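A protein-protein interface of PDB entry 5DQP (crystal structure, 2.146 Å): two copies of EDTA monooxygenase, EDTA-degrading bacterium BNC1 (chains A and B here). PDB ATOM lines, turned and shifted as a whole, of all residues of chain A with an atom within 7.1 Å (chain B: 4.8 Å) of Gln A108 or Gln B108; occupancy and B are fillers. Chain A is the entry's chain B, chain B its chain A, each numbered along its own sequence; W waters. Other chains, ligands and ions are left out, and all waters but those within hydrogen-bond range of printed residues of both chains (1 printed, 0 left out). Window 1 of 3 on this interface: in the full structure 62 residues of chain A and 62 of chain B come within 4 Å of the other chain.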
ATOM      1  N   ASP A  74      26.824  -1.656 -34.562  1.00  0.00           N
ATOM      2  CA  ASP A  74      25.983  -1.710 -33.373  1.00  0.00           C
ATOM      3  C   ASP A  74      24.730  -2.517 -33.691  1.00  0.00           C
ATOM      4  O   ASP A  74      24.052  -2.213 -34.683  1.00  0.00           O
ATOM      5  CB  ASP A  74      25.606  -0.296 -32.934  1.00  0.00           C
ATOM      6  CG  ASP A  74      24.674  -0.294 -31.756  1.00  0.00           C
ATOM      7  OD1 ASP A  74      23.444  -0.481 -31.955  1.00  0.00           O
ATOM      8  OD2 ASP A  74      25.174  -0.091 -30.635  1.00  0.00           O
ATOM      9  N   PRO A  75      24.408  -3.566 -32.910  1.00  0.00           N
ATOM     10  CA  PRO A  75      23.335  -4.496 -33.325  1.00  0.00           C
ATOM     11  C   PRO A  75      21.930  -3.916 -33.221  1.00  0.00           C
ATOM     12  O   PRO A  75      21.034  -4.387 -33.930  1.00  0.00           O
ATOM     13  CB  PRO A  75      23.517  -5.694 -32.371  1.00  0.00           C
ATOM     14  CG  PRO A  75      24.176  -5.109 -31.165  1.00  0.00           C
ATOM     15  CD  PRO A  75      25.123  -4.077 -31.724  1.00  0.00           C
ATOM     16  N   ILE A  76      21.702  -2.944 -32.340  1.00  0.00           N
ATOM     17  CA  ILE A  76      20.400  -2.285 -32.276  1.00  0.00           C
ATOM     18  C   ILE A  76      20.106  -1.557 -33.584  1.00  0.00           C
ATOM     19  O   ILE A  76      19.011  -1.677 -34.144  1.00  0.00           O
ATOM     20  CB  ILE A  76      20.328  -1.315 -31.081  1.00  0.00           C
ATOM     21  CG1 ILE A  76      20.623  -2.055 -29.760  1.00  0.00           C
ATOM     22  CG2 ILE A  76      18.929  -0.677 -31.041  1.00  0.00           C
ATOM     23  CD1 ILE A  76      20.465  -1.138 -28.483  1.00  0.00           C
ATOM     24  N   VAL A  77      21.079  -0.779 -34.070  1.00  0.00           N
ATOM     25  CA  VAL A  77      20.966  -0.105 -35.368  1.00  0.00           C
ATOM     26  C   VAL A  77      20.775  -1.122 -36.490  1.00  0.00           C
ATOM     27  O   VAL A  77      19.872  -0.997 -37.319  1.00  0.00           O
ATOM     28  CB  VAL A  77      22.205   0.781 -35.605  1.00  0.00           C
ATOM     29  CG1 VAL A  77      22.285   1.259 -37.064  1.00  0.00           C
ATOM     30  CG2 VAL A  77      22.170   1.991 -34.614  1.00  0.00           C
ATOM     31  N   PRO A 102      20.884   2.728 -18.403  1.00  0.00           N
ATOM     32  CA  PRO A 102      19.617   1.967 -18.461  1.00  0.00           C
ATOM     33  C   PRO A 102      18.492   2.671 -19.212  1.00  0.00           C
ATOM     34  O   PRO A 102      17.718   2.004 -19.907  1.00  0.00           O
ATOM     35  CB  PRO A 102      19.253   1.764 -16.984  1.00  0.00           C
ATOM     36  CG  PRO A 102      20.483   2.088 -16.206  1.00  0.00           C
ATOM     37  CD  PRO A 102      21.396   2.901 -17.035  1.00  0.00           C
ATOM     38  N   TYR A 103      18.339   3.992 -19.054  1.00  0.00           N
ATOM     39  CA  TYR A 103      17.233   4.688 -19.716  1.00  0.00           C
ATOM     40  C   TYR A 103      17.380   4.645 -21.233  1.00  0.00           C
ATOM     41  O   TYR A 103      16.394   4.451 -21.958  1.00  0.00           O
ATOM     42  CB  TYR A 103      17.148   6.150 -19.245  1.00  0.00           C
ATOM     43  CG  TYR A 103      15.866   6.842 -19.667  1.00  0.00           C
ATOM     44  CD1 TYR A 103      14.716   6.734 -18.889  1.00  0.00           C
ATOM     45  CD2 TYR A 103      15.794   7.591 -20.845  1.00  0.00           C
ATOM     46  CE1 TYR A 103      13.525   7.352 -19.266  1.00  0.00           C
ATOM     47  CE2 TYR A 103      14.586   8.216 -21.235  1.00  0.00           C
ATOM     48  CZ  TYR A 103      13.463   8.083 -20.432  1.00  0.00           C
ATOM     49  OH  TYR A 103      12.257   8.671 -20.765  1.00  0.00           O
ATOM     50  N   THR A 104      18.591   4.886 -21.731  1.00  0.00           N
ATOM     51  CA  THR A 104      18.819   4.834 -23.172  1.00  0.00           C
ATOM     52  C   THR A 104      18.565   3.434 -23.711  1.00  0.00           C
ATOM     53  O   THR A 104      17.856   3.252 -24.712  1.00  0.00           O
ATOM     54  CB  THR A 104      20.245   5.286 -23.486  1.00  0.00           C
ATOM     55  OG1 THR A 104      20.401   6.655 -23.090  1.00  0.00           O
ATOM     56  CG2 THR A 104      20.521   5.163 -24.974  1.00  0.00           C
ATOM     57  N   LEU A 105      19.138   2.424 -23.053  1.00  0.00           N
ATOM     58  CA  LEU A 105      18.969   1.058 -23.525  1.00  0.00           C
ATOM     59  C   LEU A 105      17.506   0.648 -23.495  1.00  0.00           C
ATOM     60  O   LEU A 105      17.011   0.010 -24.431  1.00  0.00           O
ATOM     61  CB  LEU A 105      19.804   0.103 -22.676  1.00  0.00           C
ATOM     62  CG  LEU A 105      19.775  -1.305 -23.292  1.00  0.00           C
ATOM     63  CD1 LEU A 105      21.072  -2.034 -23.037  1.00  0.00           C
ATOM     64  CD2 LEU A 105      18.561  -2.094 -22.727  1.00  0.00           C
ATOM     65  N   ALA A 106      16.811   0.971 -22.391  1.00  0.00           N
ATOM     66  CA  ALA A 106      15.390   0.669 -22.291  1.00  0.00           C
ATOM     67  C   ALA A 106      14.642   1.295 -23.455  1.00  0.00           C
ATOM     68  O   ALA A 106      13.782   0.657 -24.074  1.00  0.00           O
ATOM     69  CB  ALA A 106      14.830   1.169 -20.943  1.00  0.00           C
ATOM     70  N   ARG A 107      15.009   2.525 -23.811  1.00  0.00           N
ATOM     71  CA  ARG A 107      14.288   3.247 -24.855  1.00  0.00           C
ATOM     72  C   ARG A 107      14.602   2.707 -26.246  1.00  0.00           C
ATOM     73  O   ARG A 107      13.705   2.571 -27.090  1.00  0.00           O
ATOM     74  CB  ARG A 107      14.636   4.723 -24.768  1.00  0.00           C
ATOM     75  CG  ARG A 107      14.010   5.491 -25.875  1.00  0.00           C
ATOM     76  CD  ARG A 107      13.775   6.903 -25.443  1.00  0.00           C
ATOM     77  NE  ARG A 107      14.907   7.730 -25.755  1.00  0.00           N
ATOM     78  CZ  ARG A 107      14.863   8.801 -26.545  1.00  0.00           C
ATOM     79  NH1 ARG A 107      15.993   9.445 -26.778  1.00  0.00           N
ATOM     80  NH2 ARG A 107      13.719   9.221 -27.095  1.00  0.00           N
ATOM     81  N   GLN A 108      15.866   2.386 -26.503  1.00  0.00           N
ATOM     82  CA  GLN A 108      16.231   1.869 -27.819  1.00  0.00           C
ATOM     83  C   GLN A 108      15.635   0.480 -28.060  1.00  0.00           C
ATOM     84  O   GLN A 108      15.098   0.217 -29.137  1.00  0.00           O
ATOM     85  CB  GLN A 108      17.760   1.891 -27.977  1.00  0.00           C
ATOM     86  CG  GLN A 108      18.299   3.343 -28.010  1.00  0.00           C
ATOM     87  CD  GLN A 108      19.811   3.482 -28.250  1.00  0.00           C
ATOM     88  OE1 GLN A 108      20.586   2.563 -28.027  1.00  0.00           O
ATOM     89  NE2 GLN A 108      20.221   4.649 -28.729  1.00  0.00           N
ATOM     90  N   ILE A 109      15.680  -0.410 -27.068  1.00  0.00           N
ATOM     91  CA  ILE A 109      15.102  -1.747 -27.249  1.00  0.00           C
ATOM     92  C   ILE A 109      13.586  -1.670 -27.427  1.00  0.00           C
ATOM     93  O   ILE A 109      13.017  -2.310 -28.322  1.00  0.00           O
ATOM     94  CB  ILE A 109      15.472  -2.678 -26.074  1.00  0.00           C
ATOM     95  CG1 ILE A 109      16.991  -2.871 -25.969  1.00  0.00           C
ATOM     96  CG2 ILE A 109      14.742  -4.058 -26.203  1.00  0.00           C
ATOM     97  CD1 ILE A 109      17.609  -3.539 -27.164  1.00  0.00           C
ATOM     98  N   ALA A 110      12.907  -0.916 -26.555  1.00  0.00           N
ATOM     99  CA  ALA A 110      11.470  -0.692 -26.706  1.00  0.00           C
ATOM    100  C   ALA A 110      11.134  -0.055 -28.057  1.00  0.00           C
ATOM    101  O   ALA A 110      10.129  -0.409 -28.693  1.00  0.00           O
ATOM    102  CB  ALA A 110      10.973   0.189 -25.563  1.00  0.00           C
ATOM    103  N   SER A 111      11.958   0.892 -28.507  1.00  0.00           N
ATOM    104  CA  SER A 111      11.720   1.544 -29.793  1.00  0.00           C
ATOM    105  C   SER A 111      11.850   0.548 -30.934  1.00  0.00           C
ATOM    106  O   SER A 111      10.939   0.408 -31.754  1.00  0.00           O
ATOM    107  CB  SER A 111      12.690   2.704 -29.996  1.00  0.00           C
ATOM    108  OG  SER A 111      12.353   3.817 -29.183  1.00  0.00           O
ATOM    109  N   VAL A 112      12.962  -0.186 -30.989  1.00  0.00           N
ATOM    110  CA  VAL A 112      13.104  -1.086 -32.132  1.00  0.00           C
ATOM    111  C   VAL A 112      12.080  -2.206 -32.058  1.00  0.00           C
ATOM    112  O   VAL A 112      11.600  -2.696 -33.088  1.00  0.00           O
ATOM    113  CB  VAL A 112      14.540  -1.628 -32.237  1.00  0.00           C
ATOM    114  CG1 VAL A 112      14.853  -2.553 -31.073  1.00  0.00           C
ATOM    115  CG2 VAL A 112      14.730  -2.340 -33.600  1.00  0.00           C
ATOM    116  N   ASN A 113      11.715  -2.628 -30.854  1.00  0.00           N
ATOM    117  CA  ASN A 113      10.688  -3.638 -30.739  1.00  0.00           C
ATOM    118  C   ASN A 113       9.340  -3.118 -31.243  1.00  0.00           C
ATOM    119  O   ASN A 113       8.659  -3.773 -32.039  1.00  0.00           O
ATOM    120  CB  ASN A 113      10.591  -4.118 -29.285  1.00  0.00           C
ATOM    121  CG  ASN A 113       9.580  -5.207 -29.132  1.00  0.00           C
ATOM    122  OD1 ASN A 113       9.675  -6.256 -29.792  1.00  0.00           O
ATOM    123  ND2 ASN A 113       8.598  -4.980 -28.263  1.00  0.00           N
ATOM    124  N   LEU A 114       8.932  -1.946 -30.785  1.00  0.00           N
ATOM    125  CA  LEU A 114       7.630  -1.426 -31.196  1.00  0.00           C
ATOM    126  C   LEU A 114       7.622  -1.038 -32.674  1.00  0.00           C
ATOM    127  O   LEU A 114       6.645  -1.296 -33.384  1.00  0.00           O
ATOM    128  CB  LEU A 114       7.268  -0.244 -30.293  1.00  0.00           C
ATOM    129  CG  LEU A 114       5.900   0.423 -30.328  1.00  0.00           C
ATOM    130  CD1 LEU A 114       4.788  -0.590 -30.055  1.00  0.00           C
ATOM    131  CD2 LEU A 114       5.885   1.557 -29.300  1.00  0.00           C
ATOM    132  N   ILE A 120      11.427  -7.820 -31.635  1.00  0.00           N
ATOM    133  CA  ILE A 120      12.823  -7.646 -31.221  1.00  0.00           C
ATOM    134  C   ILE A 120      12.986  -7.989 -29.751  1.00  0.00           C
ATOM    135  O   ILE A 120      12.303  -7.410 -28.899  1.00  0.00           O
ATOM    136  CB  ILE A 120      13.327  -6.215 -31.485  1.00  0.00           C
ATOM    137  CG1 ILE A 120      13.370  -5.922 -32.988  1.00  0.00           C
ATOM    138  CG2 ILE A 120      14.712  -6.018 -30.853  1.00  0.00           C
ATOM    139  CD1 ILE A 120      14.168  -6.905 -33.736  1.00  0.00           C
ATOM    140  N   TRP A 161      10.001  -0.001 -19.001  1.00  0.00           N
ATOM    141  CA  TRP A 161       9.059  -0.515 -19.993  1.00  0.00           C
ATOM    142  C   TRP A 161       7.617  -0.480 -19.514  1.00  0.00           C
ATOM    143  O   TRP A 161       6.697  -0.341 -20.331  1.00  0.00           O
ATOM    144  CB  TRP A 161       9.414  -1.944 -20.368  1.00  0.00           C
ATOM    145  CG  TRP A 161      10.651  -2.057 -21.192  1.00  0.00           C
ATOM    146  CD1 TRP A 161      11.249  -1.082 -21.940  1.00  0.00           C
ATOM    147  CD2 TRP A 161      11.424  -3.244 -21.382  1.00  0.00           C
ATOM    148  NE1 TRP A 161      12.350  -1.597 -22.593  1.00  0.00           N
ATOM    149  CE2 TRP A 161      12.479  -2.921 -22.267  1.00  0.00           C
ATOM    150  CE3 TRP A 161      11.306  -4.554 -20.913  1.00  0.00           C
ATOM    151  CZ2 TRP A 161      13.444  -3.851 -22.645  1.00  0.00           C
ATOM    152  CZ3 TRP A 161      12.277  -5.495 -21.307  1.00  0.00           C
ATOM    153  CH2 TRP A 161      13.316  -5.134 -22.162  1.00  0.00           C
ATOM    154  N   LEU A 198       9.600   6.216 -18.976  1.00  0.00           N
ATOM    155  CA  LEU A 198      10.130   6.019 -20.318  1.00  0.00           C
ATOM    156  C   LEU A 198       9.242   6.706 -21.349  1.00  0.00           C
ATOM    157  O   LEU A 198       8.038   6.840 -21.166  1.00  0.00           O
ATOM    158  CB  LEU A 198      10.201   4.535 -20.654  1.00  0.00           C
ATOM    159  CG  LEU A 198      11.156   4.114 -21.778  1.00  0.00           C
ATOM    160  CD1 LEU A 198      12.598   4.397 -21.395  1.00  0.00           C
ATOM    161  CD2 LEU A 198      10.953   2.633 -22.039  1.00  0.00           C
ATOM    162  N   VAL A 200       8.683   5.620 -24.376  1.00  0.00           N
ATOM    163  CA  VAL A 200       8.166   4.645 -25.326  1.00  0.00           C
ATOM    164  C   VAL A 200       7.082   3.849 -24.605  1.00  0.00           C
ATOM    165  O   VAL A 200       7.313   3.353 -23.491  1.00  0.00           O
ATOM    166  CB  VAL A 200       9.283   3.729 -25.869  1.00  0.00           C
ATOM    167  CG1 VAL A 200       8.723   2.876 -26.974  1.00  0.00           C
ATOM    168  CG2 VAL A 200      10.440   4.546 -26.372  1.00  0.00           C
ATOM    169  N   ASP B  74      13.330   6.524 -29.902  1.00  0.00           N
ATOM    170  CA  ASP B  74      14.734   6.878 -30.053  1.00  0.00           C
ATOM    171  C   ASP B  74      15.017   7.228 -31.509  1.00  0.00           C
ATOM    172  O   ASP B  74      14.624   6.475 -32.411  1.00  0.00           O
ATOM    173  CB  ASP B  74      15.660   5.744 -29.621  1.00  0.00           C
ATOM    174  CG  ASP B  74      17.130   6.148 -29.706  1.00  0.00           C
ATOM    175  OD1 ASP B  74      17.702   6.054 -30.817  1.00  0.00           O
ATOM    176  OD2 ASP B  74      17.702   6.593 -28.681  1.00  0.00           O
ATOM    177  N   ILE B  76      17.882   7.508 -33.349  1.00  0.00           N
ATOM    178  CA  ILE B  76      18.848   6.671 -34.067  1.00  0.00           C
ATOM    179  C   ILE B  76      18.165   5.400 -34.568  1.00  0.00           C
ATOM    180  O   ILE B  76      18.306   5.021 -35.737  1.00  0.00           O
ATOM    181  CB  ILE B  76      20.067   6.358 -33.169  1.00  0.00           C
ATOM    182  CG1 ILE B  76      20.710   7.656 -32.644  1.00  0.00           C
ATOM    183  CG2 ILE B  76      21.126   5.588 -33.932  1.00  0.00           C
ATOM    184  CD1 ILE B  76      21.921   7.444 -31.683  1.00  0.00           C
ATOM    185  N   VAL B  77      17.376   4.748 -33.699  1.00  0.00           N
ATOM    186  CA  VAL B  77      16.613   3.546 -34.078  1.00  0.00           C
ATOM    187  C   VAL B  77      15.618   3.857 -35.196  1.00  0.00           C
ATOM    188  O   VAL B  77      15.569   3.162 -36.222  1.00  0.00           O
ATOM    189  CB  VAL B  77      15.905   2.976 -32.832  1.00  0.00           C
ATOM    190  CG1 VAL B  77      14.813   1.971 -33.182  1.00  0.00           C
ATOM    191  CG2 VAL B  77      16.928   2.392 -31.871  1.00  0.00           C
ATOM    192  N   THR B 104      29.603   4.632 -27.409  1.00  0.00           N
ATOM    193  CA  THR B 104      28.316   4.172 -27.902  1.00  0.00           C
ATOM    194  C   THR B 104      27.757   5.115 -28.964  1.00  0.00           C
ATOM    195  O   THR B 104      27.365   4.679 -30.052  1.00  0.00           O
ATOM    196  CB  THR B 104      27.352   4.029 -26.736  1.00  0.00           C
ATOM    197  OG1 THR B 104      27.868   3.031 -25.842  1.00  0.00           O
ATOM    198  CG2 THR B 104      25.993   3.592 -27.252  1.00  0.00           C
ATOM    199  N   LEU B 105      27.735   6.413 -28.685  1.00  0.00           N
ATOM    200  CA  LEU B 105      27.181   7.353 -29.658  1.00  0.00           C
ATOM    201  C   LEU B 105      27.991   7.368 -30.953  1.00  0.00           C
ATOM    202  O   LEU B 105      27.421   7.335 -32.051  1.00  0.00           O
ATOM    203  CB  LEU B 105      27.103   8.753 -29.053  1.00  0.00           C
ATOM    204  CG  LEU B 105      26.398   9.775 -29.948  1.00  0.00           C
ATOM    205  CD1 LEU B 105      25.717  10.802 -29.118  1.00  0.00           C
ATOM    206  CD2 LEU B 105      27.426  10.449 -30.875  1.00  0.00           C
ATOM    207  N   ALA B 106      29.325   7.437 -30.851  1.00  0.00           N
ATOM    208  CA  ALA B 106      30.166   7.405 -32.054  1.00  0.00           C
ATOM    209  C   ALA B 106      29.828   6.191 -32.921  1.00  0.00           C
ATOM    210  O   ALA B 106      29.669   6.283 -34.149  1.00  0.00           O
ATOM    211  CB  ALA B 106      31.651   7.380 -31.652  1.00  0.00           C
ATOM    212  N   ARG B 107      29.703   5.042 -32.268  1.00  0.00           N
ATOM    213  CA  ARG B 107      29.494   3.772 -32.935  1.00  0.00           C
ATOM    214  C   ARG B 107      28.089   3.662 -33.529  1.00  0.00           C
ATOM    215  O   ARG B 107      27.905   3.097 -34.615  1.00  0.00           O
ATOM    216  CB  ARG B 107      29.758   2.674 -31.915  1.00  0.00           C
ATOM    217  CG  ARG B 107      29.051   1.417 -32.164  1.00  0.00           C
ATOM    218  CD  ARG B 107      29.411   0.394 -31.117  1.00  0.00           C
ATOM    219  NE  ARG B 107      29.549  -0.894 -31.768  1.00  0.00           N
ATOM    220  CZ  ARG B 107      29.190  -2.044 -31.225  1.00  0.00           C
ATOM    221  NH1 ARG B 107      29.366  -3.159 -31.907  1.00  0.00           N
ATOM    222  NH2 ARG B 107      28.656  -2.076 -30.007  1.00  0.00           N
ATOM    223  N   GLN B 108      27.088   4.216 -32.846  1.00  0.00           N
ATOM    224  CA  GLN B 108      25.723   4.108 -33.342  1.00  0.00           C
ATOM    225  C   GLN B 108      25.463   5.078 -34.500  1.00  0.00           C
ATOM    226  O   GLN B 108      24.852   4.695 -35.502  1.00  0.00           O
ATOM    227  CB  GLN B 108      24.747   4.320 -32.188  1.00  0.00           C
ATOM    228  CG  GLN B 108      24.687   3.133 -31.251  1.00  0.00           C
ATOM    229  CD  GLN B 108      23.601   3.290 -30.196  1.00  0.00           C
ATOM    230  OE1 GLN B 108      23.187   4.406 -29.894  1.00  0.00           O
ATOM    231  NE2 GLN B 108      23.135   2.172 -29.633  1.00  0.00           N
ATOM    232  N   ILE B 109      25.956   6.312 -34.414  1.00  0.00           N
ATOM    233  CA  ILE B 109      25.844   7.210 -35.568  1.00  0.00           C
ATOM    234  C   ILE B 109      26.669   6.684 -36.747  1.00  0.00           C
ATOM    235  O   ILE B 109      26.243   6.763 -37.903  1.00  0.00           O
ATOM    236  CB  ILE B 109      26.267   8.644 -35.192  1.00  0.00           C
ATOM    237  CG1 ILE B 109      25.427   9.176 -34.022  1.00  0.00           C
ATOM    238  CG2 ILE B 109      26.232   9.582 -36.435  1.00  0.00           C
ATOM    239  CD1 ILE B 109      23.956   9.323 -34.320  1.00  0.00           C
ATOM    240  N   ALA B 110      27.870   6.174 -36.479  1.00  0.00           N
ATOM    241  CA  ALA B 110      28.713   5.682 -37.570  1.00  0.00           C
ATOM    242  C   ALA B 110      28.110   4.443 -38.208  1.00  0.00           C
ATOM    243  O   ALA B 110      28.218   4.252 -39.427  1.00  0.00           O
ATOM    244  CB  ALA B 110      30.128   5.387 -37.068  1.00  0.00           C
ATOM    245  N   SER B 111      27.457   3.599 -37.409  1.00  0.00           N
ATOM    246  CA  SER B 111      26.798   2.427 -37.963  1.00  0.00           C
ATOM    247  C   SER B 111      25.647   2.833 -38.862  1.00  0.00           C
ATOM    248  O   SER B 111      25.479   2.277 -39.948  1.00  0.00           O
ATOM    249  CB  SER B 111      26.264   1.506 -36.854  1.00  0.00           C
ATOM    250  OG  SER B 111      27.269   1.077 -35.964  1.00  0.00           O
ATOM    251  N   VAL B 112      24.799   3.758 -38.399  1.00  0.00           N
ATOM    252  CA  VAL B 112      23.613   4.030 -39.183  1.00  0.00           C
ATOM    253  C   VAL B 112      24.011   4.771 -40.442  1.00  0.00           C
ATOM    254  O   VAL B 112      23.401   4.582 -41.507  1.00  0.00           O
ATOM    255  CB  VAL B 112      22.541   4.780 -38.359  1.00  0.00           C
ATOM    256  CG1 VAL B 112      22.934   6.244 -38.111  1.00  0.00           C
ATOM    257  CG2 VAL B 112      21.191   4.673 -39.053  1.00  0.00           C
HETATM  258  O   HOH W   1      30.124  -2.046 -34.523  1.00  0.00           O
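The side-chain hydroxyl (OG) of Ser B111 sits at hydrogen-bond distance from the backbone NH (N) of Asp A74 (3.1 Å).
The side-chain amide nitrogen (NE2) of Gln A108 is in hydrogen-bond range of the side-chain carboxylate (OD2) of Asp B74.
The backbone NH of Asp B74 lies within hydrogen-bond range of the side-chain hydroxyl of Ser A111 (3.0 Å).
The side-chain carboxylate of Asp A74 sits at hydrogen-bond distance from the side-chain amide nitrogen of Gln B108.
NH1 of Arg A107 is in salt-bridge range of OD2 of Asp B74.
The side-chain amide oxygen (OE1) of Gln A108 sits at hydrogen-bond distance from the side-chain amide nitrogen (NE2) of Gln B108, at 3.0 Å.
The side-chain carboxylate (OD1) of Asp A74 lies within hydrogen-bond range of the backbone NH (N) of Ile A76.
The backbone carbonyl oxygen of Arg A107 lies within hydrogen-bond range of the side-chain hydroxyl of Ser A111 (2.8 Å).
The backbone NH of Val A77 is in hydrogen-bond range of the side-chain carboxylate of Asp A74, at 3.2 Å.
OD1 of Asp B74 lies within hydrogen-bond range of N of Ile B76, at 2.9 Å.
O of Arg B107 sits at hydrogen-bond distance from OG of Ser B111 (2.5 Å).
The side-chain carboxylate of Asp B74 sits at hydrogen-bond distance from the backbone NH of Val B77 (3.2 Å).
Among the printed residues, merely in contact across the chains: Asp A74 with Arg B107 (3.9 Å), Ile A76 with Val B77 (3.8 Å), Val A77 with Ile B76 (3.8 Å), Val A77 with Gln B108 (3.9 Å), Val A77 with Ser B111 (3.99 Å), Val A77 with Val B112 (3.7 Å), Gln A108 with Val B77 (3.9 Å), Ser A111 with Val B77 (3.9 Å) and Val A112 with Val B77 (3.6 Å).
Printed residues of chain B within 4 Å of Gln A108: Asp B74, Val B77 and Gln B108.
Of chain A, only Asp A74, Val A77 and Gln A108 come within 4 Å of Gln B108.
Of the printed residues of chain B, Val A112 touches Val B77 (3.6 Å).
Printed residues of chain A within 4 Å of Val B77: Ile A76 (3.8 Å), Gln A108 (3.9 Å), Ser A111 (3.9 Å) and Val A112 (3.6 Å).
Pro A102 touches none of the printed residues of chain B.
The nearest residue of chain A that does not touch Gln B108 is Ile A76 (4.4 Å).
The nearest printed residue of chain B that does not touch Ser A111 is Ile B76 (7.6 Å).
Printed residues of chain B that touch a printed residue of chain A: Asp B74, Ile B76, Val B77, Arg B107, Gln B108, Ser B111 and Val B112.
Hydrophobic or aromatic side chains of chain B within 4 Å of the printed part of chain A: Ile B76, Val B77 and Val B112.
Among the printed residues, 15 pairs touch across the chains.
Asp A74 touches Arg B107, and with the chains exchanged Arg A107 touches Asp B74.
Asp A74 touches Ser B111, and with the chains exchanged Ser A111 touches Asp B74.
Val A77 touches Gln B108, and with the chains exchanged Gln A108 touches Val B77.
Gln B108 touches its own counterpart, Gln A108.
Positions printed for both chains: 74, 76, 77, 104, 105, 106, 107, 108, 109, 110, 111 and 112.
Of the 15 pairs that touch across the chains among the printed residues, 15 have their exchanged pair printed and touching as well.
Water W1 bridges the guanidinium group of Arg B107 (2.9 Å) and the backbone NH of Asp A74 (3.3 Å).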
